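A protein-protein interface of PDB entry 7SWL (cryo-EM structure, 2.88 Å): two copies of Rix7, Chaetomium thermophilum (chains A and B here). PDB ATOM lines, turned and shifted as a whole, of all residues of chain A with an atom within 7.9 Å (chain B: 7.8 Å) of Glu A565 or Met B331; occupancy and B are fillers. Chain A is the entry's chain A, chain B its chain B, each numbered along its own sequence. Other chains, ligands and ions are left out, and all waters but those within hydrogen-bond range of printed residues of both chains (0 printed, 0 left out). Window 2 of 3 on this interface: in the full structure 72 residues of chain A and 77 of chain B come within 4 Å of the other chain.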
ATOM      1  N   GLN A 557      23.289 -25.862   7.089  1.00  0.00           N
ATOM      2  CA  GLN A 557      21.853 -26.081   7.226  1.00  0.00           C
ATOM      3  C   GLN A 557      21.088 -25.485   6.052  1.00  0.00           C
ATOM      4  O   GLN A 557      20.101 -26.067   5.588  1.00  0.00           O
ATOM      5  CB  GLN A 557      21.354 -25.492   8.542  1.00  0.00           C
ATOM      6  CG  GLN A 557      19.924 -25.863   8.875  1.00  0.00           C
ATOM      7  CD  GLN A 557      19.347 -25.015   9.987  1.00  0.00           C
ATOM      8  OE1 GLN A 557      19.391 -23.788   9.934  1.00  0.00           O
ATOM      9  NE2 GLN A 557      18.798 -25.669  11.005  1.00  0.00           N
ATOM     10  N   ALA A 558      21.518 -24.318   5.568  1.00  0.00           N
ATOM     11  CA  ALA A 558      20.876 -23.717   4.405  1.00  0.00           C
ATOM     12  C   ALA A 558      21.040 -24.594   3.170  1.00  0.00           C
ATOM     13  O   ALA A 558      20.105 -24.740   2.376  1.00  0.00           O
ATOM     14  CB  ALA A 558      21.447 -22.323   4.153  1.00  0.00           C
ATOM     15  N   ALA A 559      22.227 -25.174   2.986  1.00  0.00           N
ATOM     16  CA  ALA A 559      22.441 -26.086   1.867  1.00  0.00           C
ATOM     17  C   ALA A 559      21.588 -27.339   2.005  1.00  0.00           C
ATOM     18  O   ALA A 559      21.065 -27.853   1.010  1.00  0.00           O
ATOM     19  CB  ALA A 559      23.920 -26.451   1.761  1.00  0.00           C
ATOM     20  N   ALA A 560      21.446 -27.854   3.229  1.00  0.00           N
ATOM     21  CA  ALA A 560      20.603 -29.025   3.443  1.00  0.00           C
ATOM     22  C   ALA A 560      19.145 -28.721   3.125  1.00  0.00           C
ATOM     23  O   ALA A 560      18.450 -29.543   2.519  1.00  0.00           O
ATOM     24  CB  ALA A 560      20.745 -29.516   4.882  1.00  0.00           C
ATOM     25  N   GLN A 561      18.662 -27.546   3.534  1.00  0.00           N
ATOM     26  CA  GLN A 561      17.295 -27.155   3.207  1.00  0.00           C
ATOM     27  C   GLN A 561      17.121 -26.962   1.707  1.00  0.00           C
ATOM     28  O   GLN A 561      16.084 -27.331   1.145  1.00  0.00           O
ATOM     29  CB  GLN A 561      16.919 -25.882   3.961  1.00  0.00           C
ATOM     30  CG  GLN A 561      16.842 -26.064   5.464  1.00  0.00           C
ATOM     31  CD  GLN A 561      16.482 -24.789   6.189  1.00  0.00           C
ATOM     32  OE1 GLN A 561      16.652 -23.691   5.661  1.00  0.00           O
ATOM     33  NE2 GLN A 561      15.975 -24.926   7.407  1.00  0.00           N
ATOM     34  N   ALA A 562      18.122 -26.381   1.043  1.00  0.00           N
ATOM     35  CA  ALA A 562      18.058 -26.227  -0.405  1.00  0.00           C
ATOM     36  C   ALA A 562      18.017 -27.574  -1.110  1.00  0.00           C
ATOM     37  O   ALA A 562      17.429 -27.693  -2.191  1.00  0.00           O
ATOM     38  CB  ALA A 562      19.247 -25.405  -0.899  1.00  0.00           C
ATOM     39  N   CYS A 563      18.645 -28.596  -0.525  1.00  0.00           N
ATOM     40  CA  CYS A 563      18.572 -29.938  -1.091  1.00  0.00           C
ATOM     41  C   CYS A 563      17.152 -30.489  -1.036  1.00  0.00           C
ATOM     42  O   CYS A 563      16.678 -31.092  -2.005  1.00  0.00           O
ATOM     43  CB  CYS A 563      19.534 -30.868  -0.356  1.00  0.00           C
ATOM     44  SG  CYS A 563      19.349 -32.612  -0.779  1.00  0.00           S
ATOM     45  N   LEU A 564      16.459 -30.289   0.087  1.00  0.00           N
ATOM     46  CA  LEU A 564      15.117 -30.842   0.237  1.00  0.00           C
ATOM     47  C   LEU A 564      14.128 -30.179  -0.714  1.00  0.00           C
ATOM     48  O   LEU A 564      13.219 -30.841  -1.229  1.00  0.00           O
ATOM     49  CB  LEU A 564      14.652 -30.704   1.685  1.00  0.00           C
ATOM     50  CG  LEU A 564      15.393 -31.581   2.691  1.00  0.00           C
ATOM     51  CD1 LEU A 564      14.825 -31.395   4.079  1.00  0.00           C
ATOM     52  CD2 LEU A 564      15.319 -33.037   2.278  1.00  0.00           C
ATOM     53  N   GLU A 565      14.276 -28.875  -0.950  1.00  0.00           N
ATOM     54  CA  GLU A 565      13.424 -28.207  -1.929  1.00  0.00           C
ATOM     55  C   GLU A 565      13.638 -28.786  -3.320  1.00  0.00           C
ATOM     56  O   GLU A 565      12.679 -28.988  -4.074  1.00  0.00           O
ATOM     57  CB  GLU A 565      13.694 -26.704  -1.927  1.00  0.00           C
ATOM     58  CG  GLU A 565      13.421 -26.026  -0.599  1.00  0.00           C
ATOM     59  CD  GLU A 565      13.712 -24.542  -0.633  1.00  0.00           C
ATOM     60  OE1 GLU A 565      13.913 -24.002  -1.740  1.00  0.00           O
ATOM     61  OE2 GLU A 565      13.744 -23.915   0.447  1.00  0.00           O
ATOM     62  N   ARG A 566      14.894 -29.052  -3.680  1.00  0.00           N
ATOM     63  CA  ARG A 566      15.182 -29.715  -4.947  1.00  0.00           C
ATOM     64  C   ARG A 566      14.624 -31.132  -4.962  1.00  0.00           C
ATOM     65  O   ARG A 566      14.105 -31.592  -5.985  1.00  0.00           O
ATOM     66  CB  ARG A 566      16.689 -29.720  -5.196  1.00  0.00           C
ATOM     67  CG  ARG A 566      17.112 -30.376  -6.491  1.00  0.00           C
ATOM     68  CD  ARG A 566      18.618 -30.313  -6.658  1.00  0.00           C
ATOM     69  NE  ARG A 566      19.315 -30.911  -5.526  1.00  0.00           N
ATOM     70  CZ  ARG A 566      19.594 -32.203  -5.418  1.00  0.00           C
ATOM     71  NH1 ARG A 566      19.241 -33.067  -6.354  1.00  0.00           N
ATOM     72  NH2 ARG A 566      20.243 -32.638  -4.342  1.00  0.00           N
ATOM     73  N   VAL A 567      14.724 -31.840  -3.835  1.00  0.00           N
ATOM     74  CA  VAL A 567      14.178 -33.191  -3.746  1.00  0.00           C
ATOM     75  C   VAL A 567      12.660 -33.170  -3.879  1.00  0.00           C
ATOM     76  O   VAL A 567      12.072 -34.025  -4.553  1.00  0.00           O
ATOM     77  CB  VAL A 567      14.627 -33.860  -2.433  1.00  0.00           C
ATOM     78  CG1 VAL A 567      13.779 -35.087  -2.135  1.00  0.00           C
ATOM     79  CG2 VAL A 567      16.096 -34.237  -2.510  1.00  0.00           C
ATOM     80  N   TYR A 568      12.001 -32.198  -3.243  1.00  0.00           N
ATOM     81  CA  TYR A 568      10.543 -32.124  -3.309  1.00  0.00           C
ATOM     82  C   TYR A 568      10.060 -31.957  -4.744  1.00  0.00           C
ATOM     83  O   TYR A 568       9.096 -32.608  -5.162  1.00  0.00           O
ATOM     84  CB  TYR A 568      10.033 -30.971  -2.445  1.00  0.00           C
ATOM     85  CG  TYR A 568      10.000 -31.265  -0.963  1.00  0.00           C
ATOM     86  CD1 TYR A 568       9.922 -32.568  -0.492  1.00  0.00           C
ATOM     87  CD2 TYR A 568      10.039 -30.234  -0.033  1.00  0.00           C
ATOM     88  CE1 TYR A 568       9.887 -32.836   0.863  1.00  0.00           C
ATOM     89  CE2 TYR A 568      10.006 -30.492   1.322  1.00  0.00           C
ATOM     90  CZ  TYR A 568       9.929 -31.794   1.766  1.00  0.00           C
ATOM     91  OH  TYR A 568       9.894 -32.051   3.115  1.00  0.00           O
ATOM     92  N   THR A 569      10.716 -31.086  -5.513  1.00  0.00           N
ATOM     93  CA  THR A 569      10.360 -30.939  -6.920  1.00  0.00           C
ATOM     94  C   THR A 569      10.834 -32.131  -7.741  1.00  0.00           C
ATOM     95  O   THR A 569      10.226 -32.458  -8.767  1.00  0.00           O
ATOM     96  CB  THR A 569      10.947 -29.646  -7.481  1.00  0.00           C
ATOM     97  OG1 THR A 569      12.374 -29.750  -7.533  1.00  0.00           O
ATOM     98  CG2 THR A 569      10.565 -28.469  -6.600  1.00  0.00           C
ATOM     99  N   GLN A 570      11.915 -32.786  -7.310  1.00  0.00           N
ATOM    100  CA  GLN A 570      12.414 -33.954  -8.028  1.00  0.00           C
ATOM    101  C   GLN A 570      11.410 -35.097  -7.989  1.00  0.00           C
ATOM    102  O   GLN A 570      11.231 -35.810  -8.982  1.00  0.00           O
ATOM    103  CB  GLN A 570      13.753 -34.397  -7.439  1.00  0.00           C
ATOM    104  CG  GLN A 570      14.467 -35.472  -8.239  1.00  0.00           C
ATOM    105  CD  GLN A 570      15.103 -34.933  -9.506  1.00  0.00           C
ATOM    106  OE1 GLN A 570      15.231 -33.721  -9.684  1.00  0.00           O
ATOM    107  NE2 GLN A 570      15.507 -35.833 -10.395  1.00  0.00           N
ATOM    108  N   ARG A 571      10.745 -35.288  -6.851  1.00  0.00           N
ATOM    109  CA  ARG A 571       9.797 -36.381  -6.687  1.00  0.00           C
ATOM    110  C   ARG A 571       8.409 -36.052  -7.222  1.00  0.00           C
ATOM    111  O   ARG A 571       7.529 -36.917  -7.188  1.00  0.00           O
ATOM    112  CB  ARG A 571       9.697 -36.783  -5.211  1.00  0.00           C
ATOM    113  CG  ARG A 571       8.948 -35.794  -4.338  1.00  0.00           C
ATOM    114  CD  ARG A 571       8.895 -36.271  -2.896  1.00  0.00           C
ATOM    115  NE  ARG A 571       8.124 -35.372  -2.046  1.00  0.00           N
ATOM    116  CZ  ARG A 571       7.997 -35.507  -0.734  1.00  0.00           C
ATOM    117  NH1 ARG A 571       8.585 -36.496  -0.080  1.00  0.00           N
ATOM    118  NH2 ARG A 571       7.261 -34.628  -0.059  1.00  0.00           N
ATOM    119  N   PRO A 589      17.989 -37.909  -0.519  1.00  0.00           N
ATOM    120  CA  PRO A 589      18.474 -36.520  -0.532  1.00  0.00           C
ATOM    121  C   PRO A 589      19.949 -36.456  -0.160  1.00  0.00           C
ATOM    122  O   PRO A 589      20.359 -36.943   0.895  1.00  0.00           O
ATOM    123  CB  PRO A 589      17.594 -35.830   0.515  1.00  0.00           C
ATOM    124  CG  PRO A 589      17.222 -36.924   1.458  1.00  0.00           C
ATOM    125  CD  PRO A 589      17.107 -38.177   0.630  1.00  0.00           C
ATOM    126  N   ASP A 595      23.628 -26.979  -4.388  1.00  0.00           N
ATOM    127  CA  ASP A 595      22.937 -26.539  -3.180  1.00  0.00           C
ATOM    128  C   ASP A 595      23.793 -25.565  -2.382  1.00  0.00           C
ATOM    129  O   ASP A 595      23.269 -24.627  -1.772  1.00  0.00           O
ATOM    130  CB  ASP A 595      22.554 -27.744  -2.325  1.00  0.00           C
ATOM    131  CG  ASP A 595      21.618 -28.691  -3.044  1.00  0.00           C
ATOM    132  OD1 ASP A 595      20.916 -28.240  -3.972  1.00  0.00           O
ATOM    133  OD2 ASP A 595      21.581 -29.884  -2.682  1.00  0.00           O
ATOM    134  N   LYS A 598      23.562 -21.758  -3.843  1.00  0.00           N
ATOM    135  CA  LYS A 598      22.489 -20.884  -3.386  1.00  0.00           C
ATOM    136  C   LYS A 598      22.475 -20.717  -1.874  1.00  0.00           C
ATOM    137  O   LYS A 598      21.818 -19.798  -1.374  1.00  0.00           O
ATOM    138  CB  LYS A 598      21.131 -21.403  -3.864  1.00  0.00           C
ATOM    139  CG  LYS A 598      20.667 -22.679  -3.196  1.00  0.00           C
ATOM    140  CD  LYS A 598      19.218 -22.978  -3.555  1.00  0.00           C
ATOM    141  CE  LYS A 598      19.053 -23.249  -5.040  1.00  0.00           C
ATOM    142  NZ  LYS A 598      19.747 -24.498  -5.455  1.00  0.00           N
ATOM    143  N   GLU A 602      22.441 -16.684   0.417  1.00  0.00           N
ATOM    144  CA  GLU A 602      21.392 -16.313   1.357  1.00  0.00           C
ATOM    145  C   GLU A 602      21.821 -16.409   2.816  1.00  0.00           C
ATOM    146  O   GLU A 602      20.966 -16.349   3.703  1.00  0.00           O
ATOM    147  CB  GLU A 602      20.152 -17.176   1.122  1.00  0.00           C
ATOM    148  CG  GLU A 602      20.371 -18.657   1.343  1.00  0.00           C
ATOM    149  CD  GLU A 602      19.188 -19.486   0.891  1.00  0.00           C
ATOM    150  OE1 GLU A 602      18.292 -18.927   0.224  1.00  0.00           O
ATOM    151  OE2 GLU A 602      19.152 -20.695   1.200  1.00  0.00           O
ATOM    152  N   VAL B 325       7.393 -15.654   2.784  1.00  0.00           N
ATOM    153  CA  VAL B 325       7.465 -15.852   4.228  1.00  0.00           C
ATOM    154  C   VAL B 325       6.876 -17.202   4.610  1.00  0.00           C
ATOM    155  O   VAL B 325       7.371 -17.876   5.521  1.00  0.00           O
ATOM    156  CB  VAL B 325       6.762 -14.695   4.961  1.00  0.00           C
ATOM    157  CG1 VAL B 325       6.787 -14.919   6.460  1.00  0.00           C
ATOM    158  CG2 VAL B 325       7.420 -13.374   4.612  1.00  0.00           C
ATOM    159  N   ARG B 326       5.812 -17.621   3.924  1.00  0.00           N
ATOM    160  CA  ARG B 326       5.214 -18.920   4.209  1.00  0.00           C
ATOM    161  C   ARG B 326       6.174 -20.055   3.880  1.00  0.00           C
ATOM    162  O   ARG B 326       6.227 -21.059   4.598  1.00  0.00           O
ATOM    163  CB  ARG B 326       3.907 -19.076   3.432  1.00  0.00           C
ATOM    164  CG  ARG B 326       3.196 -20.392   3.682  1.00  0.00           C
ATOM    165  CD  ARG B 326       1.869 -20.451   2.952  1.00  0.00           C
ATOM    166  NE  ARG B 326       1.242 -21.760   3.079  1.00  0.00           N
ATOM    167  CZ  ARG B 326       0.038 -22.061   2.617  1.00  0.00           C
ATOM    168  NH1 ARG B 326      -0.705 -21.164   1.990  1.00  0.00           N
ATOM    169  NH2 ARG B 326      -0.435 -23.292   2.790  1.00  0.00           N
ATOM    170  N   LYS B 327       6.933 -19.920   2.789  1.00  0.00           N
ATOM    171  CA  LYS B 327       7.886 -20.962   2.420  1.00  0.00           C
ATOM    172  C   LYS B 327       8.987 -21.105   3.462  1.00  0.00           C
ATOM    173  O   LYS B 327       9.359 -22.225   3.830  1.00  0.00           O
ATOM    174  CB  LYS B 327       8.490 -20.661   1.051  1.00  0.00           C
ATOM    175  CG  LYS B 327       7.520 -20.811  -0.104  1.00  0.00           C
ATOM    176  CD  LYS B 327       8.243 -20.704  -1.434  1.00  0.00           C
ATOM    177  CE  LYS B 327       9.369 -21.720  -1.527  1.00  0.00           C
ATOM    178  NZ  LYS B 327      10.070 -21.664  -2.837  1.00  0.00           N
ATOM    179  N   LYS B 328       9.524 -19.984   3.946  1.00  0.00           N
ATOM    180  CA  LYS B 328      10.598 -20.048   4.932  1.00  0.00           C
ATOM    181  C   LYS B 328      10.106 -20.627   6.251  1.00  0.00           C
ATOM    182  O   LYS B 328      10.837 -21.360   6.924  1.00  0.00           O
ATOM    183  CB  LYS B 328      11.199 -18.660   5.144  1.00  0.00           C
ATOM    184  CG  LYS B 328      11.784 -18.049   3.887  1.00  0.00           C
ATOM    185  CD  LYS B 328      12.429 -16.707   4.174  1.00  0.00           C
ATOM    186  CE  LYS B 328      13.011 -16.096   2.913  1.00  0.00           C
ATOM    187  NZ  LYS B 328      13.713 -14.815   3.191  1.00  0.00           N
ATOM    188  N   LEU B 329       8.874 -20.302   6.643  1.00  0.00           N
ATOM    189  CA  LEU B 329       8.317 -20.871   7.864  1.00  0.00           C
ATOM    190  C   LEU B 329       7.985 -22.347   7.699  1.00  0.00           C
ATOM    191  O   LEU B 329       8.097 -23.116   8.659  1.00  0.00           O
ATOM    192  CB  LEU B 329       7.074 -20.089   8.285  1.00  0.00           C
ATOM    193  CG  LEU B 329       7.321 -18.651   8.740  1.00  0.00           C
ATOM    194  CD1 LEU B 329       6.012 -17.908   8.913  1.00  0.00           C
ATOM    195  CD2 LEU B 329       8.114 -18.640  10.031  1.00  0.00           C
ATOM    196  N   GLU B 330       7.573 -22.761   6.499  1.00  0.00           N
ATOM    197  CA  GLU B 330       7.256 -24.168   6.274  1.00  0.00           C
ATOM    198  C   GLU B 330       8.519 -25.017   6.233  1.00  0.00           C
ATOM    199  O   GLU B 330       8.517 -26.165   6.690  1.00  0.00           O
ATOM    200  CB  GLU B 330       6.454 -24.322   4.981  1.00  0.00           C
ATOM    201  CG  GLU B 330       5.722 -25.652   4.842  1.00  0.00           C
ATOM    202  CD  GLU B 330       6.594 -26.759   4.272  1.00  0.00           C
ATOM    203  OE1 GLU B 330       7.660 -26.449   3.700  1.00  0.00           O
ATOM    204  OE2 GLU B 330       6.212 -27.942   4.394  1.00  0.00           O
ATOM    205  N   MET B 331       9.605 -24.473   5.688  1.00  0.00           N
ATOM    206  CA  MET B 331      10.859 -25.214   5.615  1.00  0.00           C
ATOM    207  C   MET B 331      11.572 -25.273   6.959  1.00  0.00           C
ATOM    208  O   MET B 331      12.224 -26.277   7.265  1.00  0.00           O
ATOM    209  CB  MET B 331      11.769 -24.585   4.560  1.00  0.00           C
ATOM    210  CG  MET B 331      13.146 -25.214   4.447  1.00  0.00           C
ATOM    211  SD  MET B 331      13.104 -26.989   4.142  1.00  0.00           S
ATOM    212  CE  MET B 331      12.163 -27.050   2.623  1.00  0.00           C
ATOM    213  N   SER B 332      11.454 -24.227   7.774  1.00  0.00           N
ATOM    214  CA  SER B 332      12.210 -24.139   9.016  1.00  0.00           C
ATOM    215  C   SER B 332      11.476 -24.723  10.214  1.00  0.00           C
ATOM    216  O   SER B 332      12.124 -25.242  11.128  1.00  0.00           O
ATOM    217  CB  SER B 332      12.567 -22.681   9.311  1.00  0.00           C
ATOM    218  OG  SER B 332      13.310 -22.115   8.247  1.00  0.00           O
ATOM    219  N   ILE B 333      10.148 -24.650  10.243  1.00  0.00           N
ATOM    220  CA  ILE B 333       9.401 -25.066  11.424  1.00  0.00           C
ATOM    221  C   ILE B 333       8.395 -26.155  11.081  1.00  0.00           C
ATOM    222  O   ILE B 333       8.439 -27.250  11.650  1.00  0.00           O
ATOM    223  CB  ILE B 333       8.698 -23.865  12.080  1.00  0.00           C
ATOM    224  CG1 ILE B 333       9.736 -22.880  12.611  1.00  0.00           C
ATOM    225  CG2 ILE B 333       7.783 -24.330  13.196  1.00  0.00           C
ATOM    226  CD1 ILE B 333       9.147 -21.732  13.360  1.00  0.00           C
ATOM    227  N   ILE B 334       7.479 -25.860  10.159  1.00  0.00           N
ATOM    228  CA  ILE B 334       6.399 -26.797   9.860  1.00  0.00           C
ATOM    229  C   ILE B 334       6.951 -28.081   9.254  1.00  0.00           C
ATOM    230  O   ILE B 334       6.429 -29.174   9.501  1.00  0.00           O
ATOM    231  CB  ILE B 334       5.356 -26.129   8.947  1.00  0.00           C
ATOM    232  CG1 ILE B 334       4.704 -24.953   9.671  1.00  0.00           C
ATOM    233  CG2 ILE B 334       4.299 -27.127   8.515  1.00  0.00           C
ATOM    234  CD1 ILE B 334       3.643 -24.247   8.866  1.00  0.00           C
ATOM    235  N   GLY B 335       8.013 -27.975   8.463  1.00  0.00           N
ATOM    236  CA  GLY B 335       8.632 -29.128   7.854  1.00  0.00           C
ATOM    237  C   GLY B 335       9.168 -30.130   8.855  1.00  0.00           C
ATOM    238  O   GLY B 335       8.663 -31.250   8.970  1.00  0.00           O
ATOM    239  N   PRO B 336      10.208 -29.749   9.604  1.00  0.00           N
ATOM    240  CA  PRO B 336      10.822 -30.702  10.543  1.00  0.00           C
ATOM    241  C   PRO B 336       9.891 -31.185  11.640  1.00  0.00           C
ATOM    242  O   PRO B 336      10.148 -32.249  12.216  1.00  0.00           O
ATOM    243  CB  PRO B 336      12.006 -29.914  11.121  1.00  0.00           C
ATOM    244  CG  PRO B 336      11.711 -28.492  10.828  1.00  0.00           C
ATOM    245  CD  PRO B 336      10.957 -28.485   9.543  1.00  0.00           C
ATOM    246  N   ILE B 337       8.833 -30.445  11.963  1.00  0.00           N
ATOM    247  CA  ILE B 337       7.896 -30.914  12.977  1.00  0.00           C
ATOM    248  C   ILE B 337       7.089 -32.096  12.455  1.00  0.00           C
ATOM    249  O   ILE B 337       6.870 -33.080  13.173  1.00  0.00           O
ATOM    250  CB  ILE B 337       6.987 -29.760  13.441  1.00  0.00           C
ATOM    251  CG1 ILE B 337       7.778 -28.776  14.300  1.00  0.00           C
ATOM    252  CG2 ILE B 337       5.800 -30.290  14.222  1.00  0.00           C
ATOM    253  CD1 ILE B 337       6.952 -27.634  14.834  1.00  0.00           C
ATOM    254  N   PHE B 343      14.218 -34.576   7.613  1.00  0.00           N
ATOM    255  CA  PHE B 343      15.154 -33.493   7.880  1.00  0.00           C
ATOM    256  C   PHE B 343      16.373 -33.966   8.656  1.00  0.00           C
ATOM    257  O   PHE B 343      17.452 -33.381   8.522  1.00  0.00           O
ATOM    258  CB  PHE B 343      14.445 -32.365   8.628  1.00  0.00           C
ATOM    259  CG  PHE B 343      13.492 -31.583   7.772  1.00  0.00           C
ATOM    260  CD1 PHE B 343      12.261 -32.109   7.423  1.00  0.00           C
ATOM    261  CD2 PHE B 343      13.827 -30.324   7.315  1.00  0.00           C
ATOM    262  CE1 PHE B 343      11.387 -31.395   6.634  1.00  0.00           C
ATOM    263  CE2 PHE B 343      12.953 -29.605   6.526  1.00  0.00           C
ATOM    264  CZ  PHE B 343      11.732 -30.142   6.187  1.00  0.00           C
ATOM    265  N   ILE B 348      19.827 -31.797   9.667  1.00  0.00           N
ATOM    266  CA  ILE B 348      19.199 -30.576  10.156  1.00  0.00           C
ATOM    267  C   ILE B 348      18.755 -30.818  11.591  1.00  0.00           C
ATOM    268  O   ILE B 348      17.993 -31.753  11.862  1.00  0.00           O
ATOM    269  CB  ILE B 348      18.014 -30.150   9.277  1.00  0.00           C
ATOM    270  CG1 ILE B 348      18.500 -29.780   7.876  1.00  0.00           C
ATOM    271  CG2 ILE B 348      17.275 -28.986   9.904  1.00  0.00           C
ATOM    272  CD1 ILE B 348      17.395 -29.368   6.942  1.00  0.00           C
ATOM    273  N   ALA B 352      14.633 -24.662  15.669  1.00  0.00           N
ATOM    274  CA  ALA B 352      14.753 -23.480  14.831  1.00  0.00           C
ATOM    275  C   ALA B 352      14.583 -22.225  15.672  1.00  0.00           C
ATOM    276  O   ALA B 352      13.900 -22.231  16.698  1.00  0.00           O
ATOM    277  CB  ALA B 352      13.724 -23.481  13.697  1.00  0.00           C
ATOM    278  N   ILE B 354      13.656 -18.163  14.760  1.00  0.00           N
ATOM    279  CA  ILE B 354      13.234 -17.270  13.690  1.00  0.00           C
ATOM    280  C   ILE B 354      12.862 -15.927  14.296  1.00  0.00           C
ATOM    281  O   ILE B 354      12.141 -15.870  15.297  1.00  0.00           O
ATOM    282  CB  ILE B 354      12.052 -17.858  12.896  1.00  0.00           C
ATOM    283  CG1 ILE B 354      12.496 -19.119  12.155  1.00  0.00           C
ATOM    284  CG2 ILE B 354      11.490 -16.837  11.928  1.00  0.00           C
ATOM    285  CD1 ILE B 354      11.433 -19.716  11.278  1.00  0.00           C
ATOM    286  N   TYR B 455      11.094 -24.903  19.002  1.00  0.00           N
ATOM    287  CA  TYR B 455      11.163 -23.965  17.891  1.00  0.00           C
ATOM    288  C   TYR B 455      10.727 -22.599  18.398  1.00  0.00           C
ATOM    289  O   TYR B 455       9.635 -22.459  18.954  1.00  0.00           O
ATOM    290  CB  TYR B 455      10.284 -24.433  16.731  1.00  0.00           C
ATOM    291  CG  TYR B 455      10.710 -25.770  16.166  1.00  0.00           C
ATOM    292  CD1 TYR B 455      10.372 -26.955  16.801  1.00  0.00           C
ATOM    293  CD2 TYR B 455      11.450 -25.845  14.998  1.00  0.00           C
ATOM    294  CE1 TYR B 455      10.762 -28.173  16.293  1.00  0.00           C
ATOM    295  CE2 TYR B 455      11.845 -27.059  14.483  1.00  0.00           C
ATOM    296  CZ  TYR B 455      11.498 -28.218  15.133  1.00  0.00           C
ATOM    297  OH  TYR B 455      11.887 -29.431  14.621  1.00  0.00           O
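The side-chain hydroxyl (OG) of Ser B332 lies within hydrogen-bond range of the backbone carbonyl oxygen (O) of Lys B328.
N of Ile B348 lies within hydrogen-bond range of O of Phe B343 (3.1 Å).
No position is printed for both chains.
Printed residues of chain A that touch a printed residue of chain B: Gln A557, Ala A560, Gln A561, Leu A564, Glu A565 and Tyr A568.
Hydrophobic or aromatic side chains of chain A that line the printed part of chain B: Ala A560, Leu A564 and Tyr A568.
Printed residues of chain B that touch a printed residue of chain A: Met B331, Ser B332, Phe B343 and Ile B348.
Met B331 touches two residues of chain A.
Printed residues of chain B within 4 Å of Gln A561: Met B331, Ser B332 and Ile B348.
Of the printed residues of chain B, Gln A557 touches Ile B348.
Of the printed residues of chain A, Ile B348 touches Gln A557 (3.8 Å), Ala A560 (3.8 Å) and Gln A561 (3.7 Å).
Printed residues of chain A within 4 Å of Ser B332: Gln A561.
Of the printed residues of chain B, Tyr A568 touches Phe B343.
Leu B329 touches none of the printed residues of chain A.
The nearest residue of chain A that does not touch Met B331 is Tyr A568 (4.3 Å).
The nearest printed residue of chain B that does not touch Ala A560 is Met B331 (6.1 Å).
Among the printed residues, pairs that only touch across the chains: Leu A564 with Phe B343 (3.6 Å), Glu A565 with Met B331 (3.6 Å), Gln A561 with Ile B348 (3.7 Å), Ala A560 with Ile B348 (3.8 Å), Gln A561 with Met B331 (3.8 Å), Gln A557 with Ile B348 (3.8 Å), Tyr A568 with Phe B343 (3.9 Å) and Gln A561 with Ser B332 (3.96 Å).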
